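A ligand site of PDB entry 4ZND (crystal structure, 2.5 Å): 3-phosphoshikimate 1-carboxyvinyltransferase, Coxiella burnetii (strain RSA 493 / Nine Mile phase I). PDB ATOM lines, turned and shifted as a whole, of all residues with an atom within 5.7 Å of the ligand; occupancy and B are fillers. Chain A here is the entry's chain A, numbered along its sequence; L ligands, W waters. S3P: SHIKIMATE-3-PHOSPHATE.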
ATOM      1  N   LYS A  24     -30.808 -15.336  -0.107  1.00  0.00           N
ATOM      2  CA  LYS A  24     -29.626 -16.042  -0.589  1.00  0.00           C
ATOM      3  C   LYS A  24     -28.705 -16.469   0.571  1.00  0.00           C
ATOM      4  O   LYS A  24     -28.251 -17.607   0.645  1.00  0.00           O
ATOM      5  CB  LYS A  24     -28.878 -15.158  -1.585  1.00  0.00           C
ATOM      6  CG  LYS A  24     -27.552 -15.753  -2.016  1.00  0.00           C
ATOM      7  CD  LYS A  24     -27.108 -15.149  -3.314  1.00  0.00           C
ATOM      8  CE  LYS A  24     -26.843 -13.669  -3.172  1.00  0.00           C
ATOM      9  NZ  LYS A  24     -25.579 -13.469  -2.473  1.00  0.00           N
ATOM     10  N   SER A  25     -28.449 -15.520   1.479  1.00  0.00           N
ATOM     11  CA  SER A  25     -27.548 -15.670   2.613  1.00  0.00           C
ATOM     12  C   SER A  25     -28.037 -16.728   3.575  1.00  0.00           C
ATOM     13  O   SER A  25     -27.278 -17.616   3.980  1.00  0.00           O
ATOM     14  CB  SER A  25     -27.465 -14.343   3.347  1.00  0.00           C
ATOM     15  OG  SER A  25     -26.467 -13.546   2.765  1.00  0.00           O
ATOM     16  N   ARG A  29     -26.651 -20.968   4.292  1.00  0.00           N
ATOM     17  CA  ARG A  29     -26.459 -21.498   5.699  1.00  0.00           C
ATOM     18  C   ARG A  29     -27.405 -22.646   6.014  1.00  0.00           C
ATOM     19  O   ARG A  29     -27.000 -23.659   6.620  1.00  0.00           O
ATOM     20  CB  ARG A  29     -26.605 -20.397   6.730  1.00  0.00           C
ATOM     21  CG  ARG A  29     -25.596 -19.249   6.460  1.00  0.00           C
ATOM     22  CD  ARG A  29     -26.033 -17.947   7.118  1.00  0.00           C
ATOM     23  NE  ARG A  29     -24.979 -16.979   7.347  1.00  0.00           N
ATOM     24  CZ  ARG A  29     -24.405 -16.217   6.404  1.00  0.00           C
ATOM     25  NH1 ARG A  29     -24.792 -16.300   5.087  1.00  0.00           N
ATOM     26  NH2 ARG A  29     -23.446 -15.343   6.749  1.00  0.00           N
ATOM     27  N   THR A  99     -20.083 -16.414  -0.970  1.00  0.00           N
ATOM     28  CA  THR A  99     -20.557 -16.981   0.279  1.00  0.00           C
ATOM     29  C   THR A  99     -20.296 -18.455   0.315  1.00  0.00           C
ATOM     30  O   THR A  99     -19.807 -18.957   1.320  1.00  0.00           O
ATOM     31  CB  THR A  99     -22.035 -16.698   0.418  1.00  0.00           C
ATOM     32  OG1 THR A  99     -22.278 -15.296   0.130  1.00  0.00           O
ATOM     33  CG2 THR A  99     -22.483 -17.020   1.807  1.00  0.00           C
ATOM     34  N   ARG A 102     -16.423 -19.270   0.821  1.00  0.00           N
ATOM     35  CA  ARG A 102     -15.834 -18.859   2.122  1.00  0.00           C
ATOM     36  C   ARG A 102     -16.407 -19.750   3.237  1.00  0.00           C
ATOM     37  O   ARG A 102     -15.705 -20.147   4.155  1.00  0.00           O
ATOM     38  CB  ARG A 102     -15.996 -17.358   2.335  1.00  0.00           C
ATOM     39  CG  ARG A 102     -15.239 -16.504   1.272  1.00  0.00           C
ATOM     40  CD  ARG A 102     -14.969 -15.111   1.803  1.00  0.00           C
ATOM     41  NE  ARG A 102     -14.107 -14.210   0.981  1.00  0.00           N
ATOM     42  CZ  ARG A 102     -14.617 -13.188   0.279  1.00  0.00           C
ATOM     43  NH1 ARG A 102     -15.927 -13.040   0.278  1.00  0.00           N
ATOM     44  NH2 ARG A 102     -13.839 -12.317  -0.420  1.00  0.00           N
ATOM     45  N   LEU A 103     -17.668 -20.160   3.094  1.00  0.00           N
ATOM     46  CA  LEU A 103     -18.311 -20.981   4.109  1.00  0.00           C
ATOM     47  C   LEU A 103     -17.910 -22.405   3.965  1.00  0.00           C
ATOM     48  O   LEU A 103     -17.615 -23.059   4.979  1.00  0.00           O
ATOM     49  CB  LEU A 103     -19.793 -20.862   3.986  1.00  0.00           C
ATOM     50  CG  LEU A 103     -20.417 -19.849   4.947  1.00  0.00           C
ATOM     51  CD1 LEU A 103     -19.829 -18.475   4.750  1.00  0.00           C
ATOM     52  CD2 LEU A 103     -21.917 -19.780   4.730  1.00  0.00           C
ATOM     53  N   ARG A 126     -11.696 -12.786  -6.090  1.00  0.00           N
ATOM     54  CA  ARG A 126     -12.185 -12.235  -4.817  1.00  0.00           C
ATOM     55  C   ARG A 126     -11.236 -12.645  -3.691  1.00  0.00           C
ATOM     56  O   ARG A 126     -10.645 -13.738  -3.747  1.00  0.00           O
ATOM     57  CB  ARG A 126     -13.683 -12.596  -4.620  1.00  0.00           C
ATOM     58  CG  ARG A 126     -14.454 -11.719  -5.627  1.00  0.00           C
ATOM     59  CD  ARG A 126     -15.921 -11.956  -5.657  1.00  0.00           C
ATOM     60  NE  ARG A 126     -16.450 -11.577  -4.384  1.00  0.00           N
ATOM     61  CZ  ARG A 126     -17.653 -11.931  -3.977  1.00  0.00           C
ATOM     62  NH1 ARG A 126     -18.449 -12.656  -4.785  1.00  0.00           N
ATOM     63  NH2 ARG A 126     -18.025 -11.569  -2.765  1.00  0.00           N
ATOM     64  N   ARG A 130      -8.348 -13.078   4.229  1.00  0.00           N
ATOM     65  CA  ARG A 130      -9.201 -12.831   5.347  1.00  0.00           C
ATOM     66  C   ARG A 130      -9.722 -14.147   5.960  1.00  0.00           C
ATOM     67  O   ARG A 130     -10.038 -14.176   7.143  1.00  0.00           O
ATOM     68  CB  ARG A 130     -10.347 -11.877   4.907  1.00  0.00           C
ATOM     69  CG  ARG A 130     -11.258 -12.469   3.767  1.00  0.00           C
ATOM     70  CD  ARG A 130     -12.338 -11.521   3.265  1.00  0.00           C
ATOM     71  NE  ARG A 130     -11.780 -10.248   2.858  1.00  0.00           N
ATOM     72  CZ  ARG A 130     -12.456  -9.142   2.613  1.00  0.00           C
ATOM     73  NH1 ARG A 130     -13.771  -9.102   2.744  1.00  0.00           N
ATOM     74  NH2 ARG A 130     -11.778  -8.060   2.310  1.00  0.00           N
ATOM     75  N   ALA A 169     -15.630  -5.756   8.694  1.00  0.00           N
ATOM     76  CA  ALA A 169     -16.932  -6.191   9.183  1.00  0.00           C
ATOM     77  C   ALA A 169     -17.559  -7.247   8.207  1.00  0.00           C
ATOM     78  O   ALA A 169     -18.577  -6.981   7.551  1.00  0.00           O
ATOM     79  CB  ALA A 169     -17.847  -4.966   9.351  1.00  0.00           C
ATOM     80  N   SER A 170     -16.967  -8.451   8.163  1.00  0.00           N
ATOM     81  CA  SER A 170     -17.347  -9.501   7.197  1.00  0.00           C
ATOM     82  C   SER A 170     -18.105 -10.673   7.848  1.00  0.00           C
ATOM     83  O   SER A 170     -17.529 -11.391   8.640  1.00  0.00           O
ATOM     84  CB  SER A 170     -16.100 -10.034   6.503  1.00  0.00           C
ATOM     85  OG  SER A 170     -16.410 -11.223   5.813  1.00  0.00           O
ATOM     86  N   ALA A 171     -19.349 -10.909   7.466  1.00  0.00           N
ATOM     87  CA  ALA A 171     -20.146 -12.027   8.041  1.00  0.00           C
ATOM     88  C   ALA A 171     -19.645 -13.375   7.541  1.00  0.00           C
ATOM     89  O   ALA A 171     -19.886 -14.422   8.199  1.00  0.00           O
ATOM     90  CB  ALA A 171     -21.665 -11.894   7.779  1.00  0.00           C
ATOM     91  N   GLN A 172     -19.009 -13.347   6.361  1.00  0.00           N
ATOM     92  CA  GLN A 172     -18.530 -14.555   5.710  1.00  0.00           C
ATOM     93  C   GLN A 172     -17.325 -15.077   6.504  1.00  0.00           C
ATOM     94  O   GLN A 172     -17.223 -16.296   6.831  1.00  0.00           O
ATOM     95  CB  GLN A 172     -18.180 -14.287   4.238  1.00  0.00           C
ATOM     96  CG  GLN A 172     -19.402 -14.102   3.309  1.00  0.00           C
ATOM     97  CD  GLN A 172     -19.038 -14.008   1.839  1.00  0.00           C
ATOM     98  OE1 GLN A 172     -17.972 -14.432   1.417  1.00  0.00           O
ATOM     99  NE2 GLN A 172     -19.936 -13.486   1.053  1.00  0.00           N
ATOM    100  N   VAL A 173     -16.429 -14.143   6.846  1.00  0.00           N
ATOM    101  CA  VAL A 173     -15.302 -14.452   7.656  1.00  0.00           C
ATOM    102  C   VAL A 173     -15.842 -15.010   9.030  1.00  0.00           C
ATOM    103  O   VAL A 173     -15.519 -16.138   9.432  1.00  0.00           O
ATOM    104  CB  VAL A 173     -14.335 -13.254   7.738  1.00  0.00           C
ATOM    105  CG1 VAL A 173     -13.231 -13.530   8.720  1.00  0.00           C
ATOM    106  CG2 VAL A 173     -13.685 -12.942   6.383  1.00  0.00           C
ATOM    107  N   SER A 175     -18.682 -16.306   9.722  1.00  0.00           N
ATOM    108  CA  SER A 175     -19.372 -17.571   9.469  1.00  0.00           C
ATOM    109  C   SER A 175     -18.399 -18.734   9.196  1.00  0.00           C
ATOM    110  O   SER A 175     -18.630 -19.854   9.661  1.00  0.00           O
ATOM    111  CB  SER A 175     -20.290 -17.366   8.296  1.00  0.00           C
ATOM    112  OG  SER A 175     -21.349 -16.573   8.717  1.00  0.00           O
ATOM    113  N   ARG A 197     -24.228  -9.192   9.366  1.00  0.00           N
ATOM    114  CA  ARG A 197     -25.403 -10.097   9.341  1.00  0.00           C
ATOM    115  C   ARG A 197     -25.190 -11.430  10.164  1.00  0.00           C
ATOM    116  O   ARG A 197     -24.092 -12.085  10.162  1.00  0.00           O
ATOM    117  CB  ARG A 197     -25.859 -10.356   7.911  1.00  0.00           C
ATOM    118  CG  ARG A 197     -25.014 -11.318   7.135  1.00  0.00           C
ATOM    119  CD  ARG A 197     -25.418 -11.294   5.688  1.00  0.00           C
ATOM    120  NE  ARG A 197     -25.305  -9.951   5.113  1.00  0.00           N
ATOM    121  CZ  ARG A 197     -25.754  -9.651   3.890  1.00  0.00           C
ATOM    122  NH1 ARG A 197     -26.327 -10.631   3.175  1.00  0.00           N
ATOM    123  NH2 ARG A 197     -25.601  -8.420   3.374  1.00  0.00           N
ATOM    124  N   HIS A 199     -27.100 -14.273  10.436  1.00  0.00           N
ATOM    125  CA  HIS A 199     -27.883 -15.432  10.051  1.00  0.00           C
ATOM    126  C   HIS A 199     -27.305 -16.737  10.569  1.00  0.00           C
ATOM    127  O   HIS A 199     -28.073 -17.685  10.840  1.00  0.00           O
ATOM    128  CB  HIS A 199     -28.003 -15.507   8.515  1.00  0.00           C
ATOM    129  CG  HIS A 199     -28.583 -14.278   7.913  1.00  0.00           C
ATOM    130  ND1 HIS A 199     -29.828 -13.781   8.265  1.00  0.00           N
ATOM    131  CD2 HIS A 199     -28.069 -13.388   7.019  1.00  0.00           C
ATOM    132  CE1 HIS A 199     -30.054 -12.680   7.589  1.00  0.00           C
ATOM    133  NE2 HIS A 199     -28.995 -12.412   6.831  1.00  0.00           N
ATOM    134  N   ILE A 317     -24.476  -3.118   2.690  1.00  0.00           N
ATOM    135  CA  ILE A 317     -23.336  -3.317   1.831  1.00  0.00           C
ATOM    136  C   ILE A 317     -23.803  -3.777   0.443  1.00  0.00           C
ATOM    137  O   ILE A 317     -23.398  -3.202  -0.533  1.00  0.00           O
ATOM    138  CB  ILE A 317     -22.334  -4.264   2.505  1.00  0.00           C
ATOM    139  CG1 ILE A 317     -21.036  -4.304   1.676  1.00  0.00           C
ATOM    140  CG2 ILE A 317     -22.957  -5.655   2.794  1.00  0.00           C
ATOM    141  CD1 ILE A 317     -20.311  -2.960   1.666  1.00  0.00           C
ATOM    142  N   ASP A 318     -24.742  -4.706   0.365  1.00  0.00           N
ATOM    143  CA  ASP A 318     -25.272  -5.164  -0.931  1.00  0.00           C
ATOM    144  C   ASP A 318     -26.259  -4.187  -1.615  1.00  0.00           C
ATOM    145  O   ASP A 318     -26.469  -4.233  -2.837  1.00  0.00           O
ATOM    146  CB  ASP A 318     -25.871  -6.585  -0.788  1.00  0.00           C
ATOM    147  CG  ASP A 318     -24.779  -7.633  -0.525  1.00  0.00           C
ATOM    148  OD1 ASP A 318     -23.618  -7.466  -1.012  1.00  0.00           O
ATOM    149  OD2 ASP A 318     -25.035  -8.610   0.211  1.00  0.00           O
ATOM    150  N   GLU A 341     -14.943  -1.963   0.992  1.00  0.00           N
ATOM    151  CA  GLU A 341     -15.407  -3.326   0.759  1.00  0.00           C
ATOM    152  C   GLU A 341     -16.177  -3.532  -0.611  1.00  0.00           C
ATOM    153  O   GLU A 341     -16.195  -4.638  -1.197  1.00  0.00           O
ATOM    154  CB  GLU A 341     -16.216  -3.792   1.981  1.00  0.00           C
ATOM    155  CG  GLU A 341     -15.313  -4.340   3.086  1.00  0.00           C
ATOM    156  CD  GLU A 341     -14.684  -5.682   2.698  1.00  0.00           C
ATOM    157  OE1 GLU A 341     -15.403  -6.709   2.624  1.00  0.00           O
ATOM    158  OE2 GLU A 341     -13.486  -5.724   2.420  1.00  0.00           O
ATOM    159  N   LYS A 345     -16.079  -6.957  -4.375  1.00  0.00           N
ATOM    160  CA  LYS A 345     -17.265  -7.812  -4.621  1.00  0.00           C
ATOM    161  C   LYS A 345     -17.176  -8.520  -5.962  1.00  0.00           C
ATOM    162  O   LYS A 345     -16.084  -8.723  -6.493  1.00  0.00           O
ATOM    163  CB  LYS A 345     -18.561  -6.994  -4.485  1.00  0.00           C
ATOM    164  CG  LYS A 345     -18.741  -6.429  -3.087  1.00  0.00           C
ATOM    165  CD  LYS A 345     -18.724  -7.490  -1.977  1.00  0.00           C
ATOM    166  CE  LYS A 345     -18.991  -6.837  -0.608  1.00  0.00           C
ATOM    167  NZ  LYS A 345     -19.006  -7.716   0.610  1.00  0.00           N
ATOM    168  N   GLU A 346     -18.333  -8.939  -6.485  1.00  0.00           N
ATOM    169  CA  GLU A 346     -18.418  -9.696  -7.750  1.00  0.00           C
ATOM    170  C   GLU A 346     -17.679  -8.950  -8.812  1.00  0.00           C
ATOM    171  O   GLU A 346     -16.980  -9.530  -9.611  1.00  0.00           O
ATOM    172  CB  GLU A 346     -19.872  -9.883  -8.216  1.00  0.00           C
ATOM    173  CG  GLU A 346     -20.639 -10.994  -7.504  1.00  0.00           C
ATOM    174  CD  GLU A 346     -21.271 -10.602  -6.166  1.00  0.00           C
ATOM    175  OE1 GLU A 346     -20.678  -9.777  -5.418  1.00  0.00           O
ATOM    176  OE2 GLU A 346     -22.379 -11.166  -5.831  1.00  0.00           O
ATOM    177  N   ARG A 349     -17.673  -2.506  -7.308  1.00  0.00           N
ATOM    178  CA  ARG A 349     -19.037  -1.895  -7.430  1.00  0.00           C
ATOM    179  C   ARG A 349     -19.005  -0.391  -7.446  1.00  0.00           C
ATOM    180  O   ARG A 349     -19.874   0.199  -8.017  1.00  0.00           O
ATOM    181  CB  ARG A 349     -19.946  -2.376  -6.326  1.00  0.00           C
ATOM    182  CG  ARG A 349     -20.176  -3.877  -6.451  1.00  0.00           C
ATOM    183  CD  ARG A 349     -21.314  -4.433  -5.623  1.00  0.00           C
ATOM    184  NE  ARG A 349     -21.900  -5.656  -6.173  1.00  0.00           N
ATOM    185  CZ  ARG A 349     -22.493  -6.626  -5.463  1.00  0.00           C
ATOM    186  NH1 ARG A 349     -22.582  -6.574  -4.146  1.00  0.00           N
ATOM    187  NH2 ARG A 349     -22.983  -7.656  -6.107  1.00  0.00           N
ATOM    188  N   ARG A 390     -26.148  -7.305  -9.276  1.00  0.00           N
ATOM    189  CA  ARG A 390     -26.741  -6.171  -8.641  1.00  0.00           C
ATOM    190  C   ARG A 390     -26.476  -4.895  -9.414  1.00  0.00           C
ATOM    191  O   ARG A 390     -27.251  -3.980  -9.316  1.00  0.00           O
ATOM    192  CB  ARG A 390     -26.183  -6.071  -7.221  1.00  0.00           C
ATOM    193  CG  ARG A 390     -26.742  -7.130  -6.282  1.00  0.00           C
ATOM    194  CD  ARG A 390     -26.618  -6.721  -4.804  1.00  0.00           C
ATOM    195  NE  ARG A 390     -26.750  -7.934  -3.998  1.00  0.00           N
ATOM    196  CZ  ARG A 390     -27.875  -8.641  -3.869  1.00  0.00           C
ATOM    197  NH1 ARG A 390     -29.019  -8.240  -4.414  1.00  0.00           N
ATOM    198  NH2 ARG A 390     -27.859  -9.762  -3.177  1.00  0.00           N
HETATM  199  C1  S3P L   1     -22.864 -12.208   2.954  1.00  0.00           C
HETATM  200  C2  S3P L   1     -22.197 -11.184   3.567  1.00  0.00           C
HETATM  201  C3  S3P L   1     -21.483 -10.038   2.809  1.00  0.00           C
HETATM  202  C4  S3P L   1     -22.346  -9.771   1.568  1.00  0.00           C
HETATM  203  C5  S3P L   1     -22.516 -11.075   0.738  1.00  0.00           C
HETATM  204  C6  S3P L   1     -23.311 -12.115   1.496  1.00  0.00           C
HETATM  205  C7  S3P L   1     -23.174 -13.447   3.720  1.00  0.00           C
HETATM  206  O1  S3P L   1     -20.069 -10.336   2.508  1.00  0.00           O
HETATM  207  O2  S3P L   1     -21.772  -8.729   0.770  1.00  0.00           O
HETATM  208  O3  S3P L   1     -23.190 -10.829  -0.483  1.00  0.00           O
HETATM  209  O4  S3P L   1     -24.152 -14.184   3.390  1.00  0.00           O
HETATM  210  O5  S3P L   1     -22.468 -13.734   4.717  1.00  0.00           O
HETATM  211  P1  S3P L   1     -18.720  -9.926   3.373  1.00  0.00           P
HETATM  212  O6  S3P L   1     -17.591  -9.847   2.391  1.00  0.00           O
HETATM  213  O7  S3P L   1     -18.510 -11.003   4.415  1.00  0.00           O
HETATM  214  O8  S3P L   1     -19.100  -8.604   3.936  1.00  0.00           O
HETATM  215  O   HOH W   1     -20.594  -8.652   6.017  1.00  0.00           O
HETATM  216  O   HOH W   2     -18.313  -6.154   3.043  1.00  0.00           O
HETATM  217  O   HOH W   3     -15.520 -11.347   3.080  1.00  0.00           O
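The side-chain hydroxyl of Ser 25 sits at hydrogen-bond distance from the guanidinium group of Arg 197 (2.9 Å).
The side-chain hydroxyl (OG) of Ser 170 lies close to the backbone NH (N) of Gln 172 (3.4 Å).
The backbone NH (N) of Val 173 sits at hydrogen-bond distance from the side-chain hydroxyl (OG) of Ser 170 (3.1 Å).
The side-chain carboxylate of Asp 318 lies within salt-bridge range of the guanidinium group of Arg 197 (3.2 Å).
The side-chain hydroxyl of Thr 99 is in hydrogen-bond range of the side-chain amide nitrogen of Gln 172 (3.1 Å).
The guanidinium group of Arg 102 sits at hydrogen-bond distance from the side-chain amide oxygen of Gln 172 (2.7 Å).
The backbone carbonyl oxygen (O) of Ala 171 sits at hydrogen-bond distance from the side-chain hydroxyl (OG) of Ser 175 (2.7 Å).
NH2 of Arg 130 is in salt-bridge range of OE2 of Glu 341, at 2.9 Å.
Merely in contact with the ligand: Thr 99, Ala 169, Arg 197, Ile 317 and Glu 341.
The nearest printed residue that does not touch the ligand is Lys 24 (4.1 Å).
OG of Ser 25 is in hydrogen-bond range of O4 of the ligand (2.5 Å).
OG of Ser 170 is in hydrogen-bond range of O7 of the ligand (2.5 Å).
The guanidinium group of Arg 29 is in salt-bridge range of an oxygen (O5) of the ligand, 2.8 Å away.
The side-chain carboxylate (OD1) of Asp 318 lies within hydrogen-bond range of an oxygen (O2) of the ligand (2.9 Å).
O6 of the ligand lies within salt-bridge range of NZ of Lys 345, 3.1 Å away.
N of Gln 172 sits at hydrogen-bond distance from O7 of the ligand (3.1 Å).
An oxygen (O1) of the ligand lies within hydrogen-bond range of the side-chain amide nitrogen of Gln 172 (3.5 Å).
N of Ala 171 is in hydrogen-bond range of O7 of the ligand.
An oxygen (O6) of the ligand is in salt-bridge range of the guanidinium group (NH1) of Arg 130.
Water W1 lies within hydrogen-bond range of O8 of the ligand (2.6 Å), N of Ala 171 (3.0 Å) and O of Ala 169 (3.0 Å).
Water W3 lies within hydrogen-bond range of an oxygen (O6) of the ligand (2.6 Å), the guanidinium group (NH1) of Arg 130 (2.9 Å), the side-chain hydroxyl (OG) of Ser 170 (2.9 Å) and the guanidinium group (NH1) of Arg 102 (3.3 Å).
Water W2 lies within hydrogen-bond range of O8 of the ligand (2.7 Å), NZ of Lys 345 (3.0 Å) and OE1 of Glu 341 (3.0 Å).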
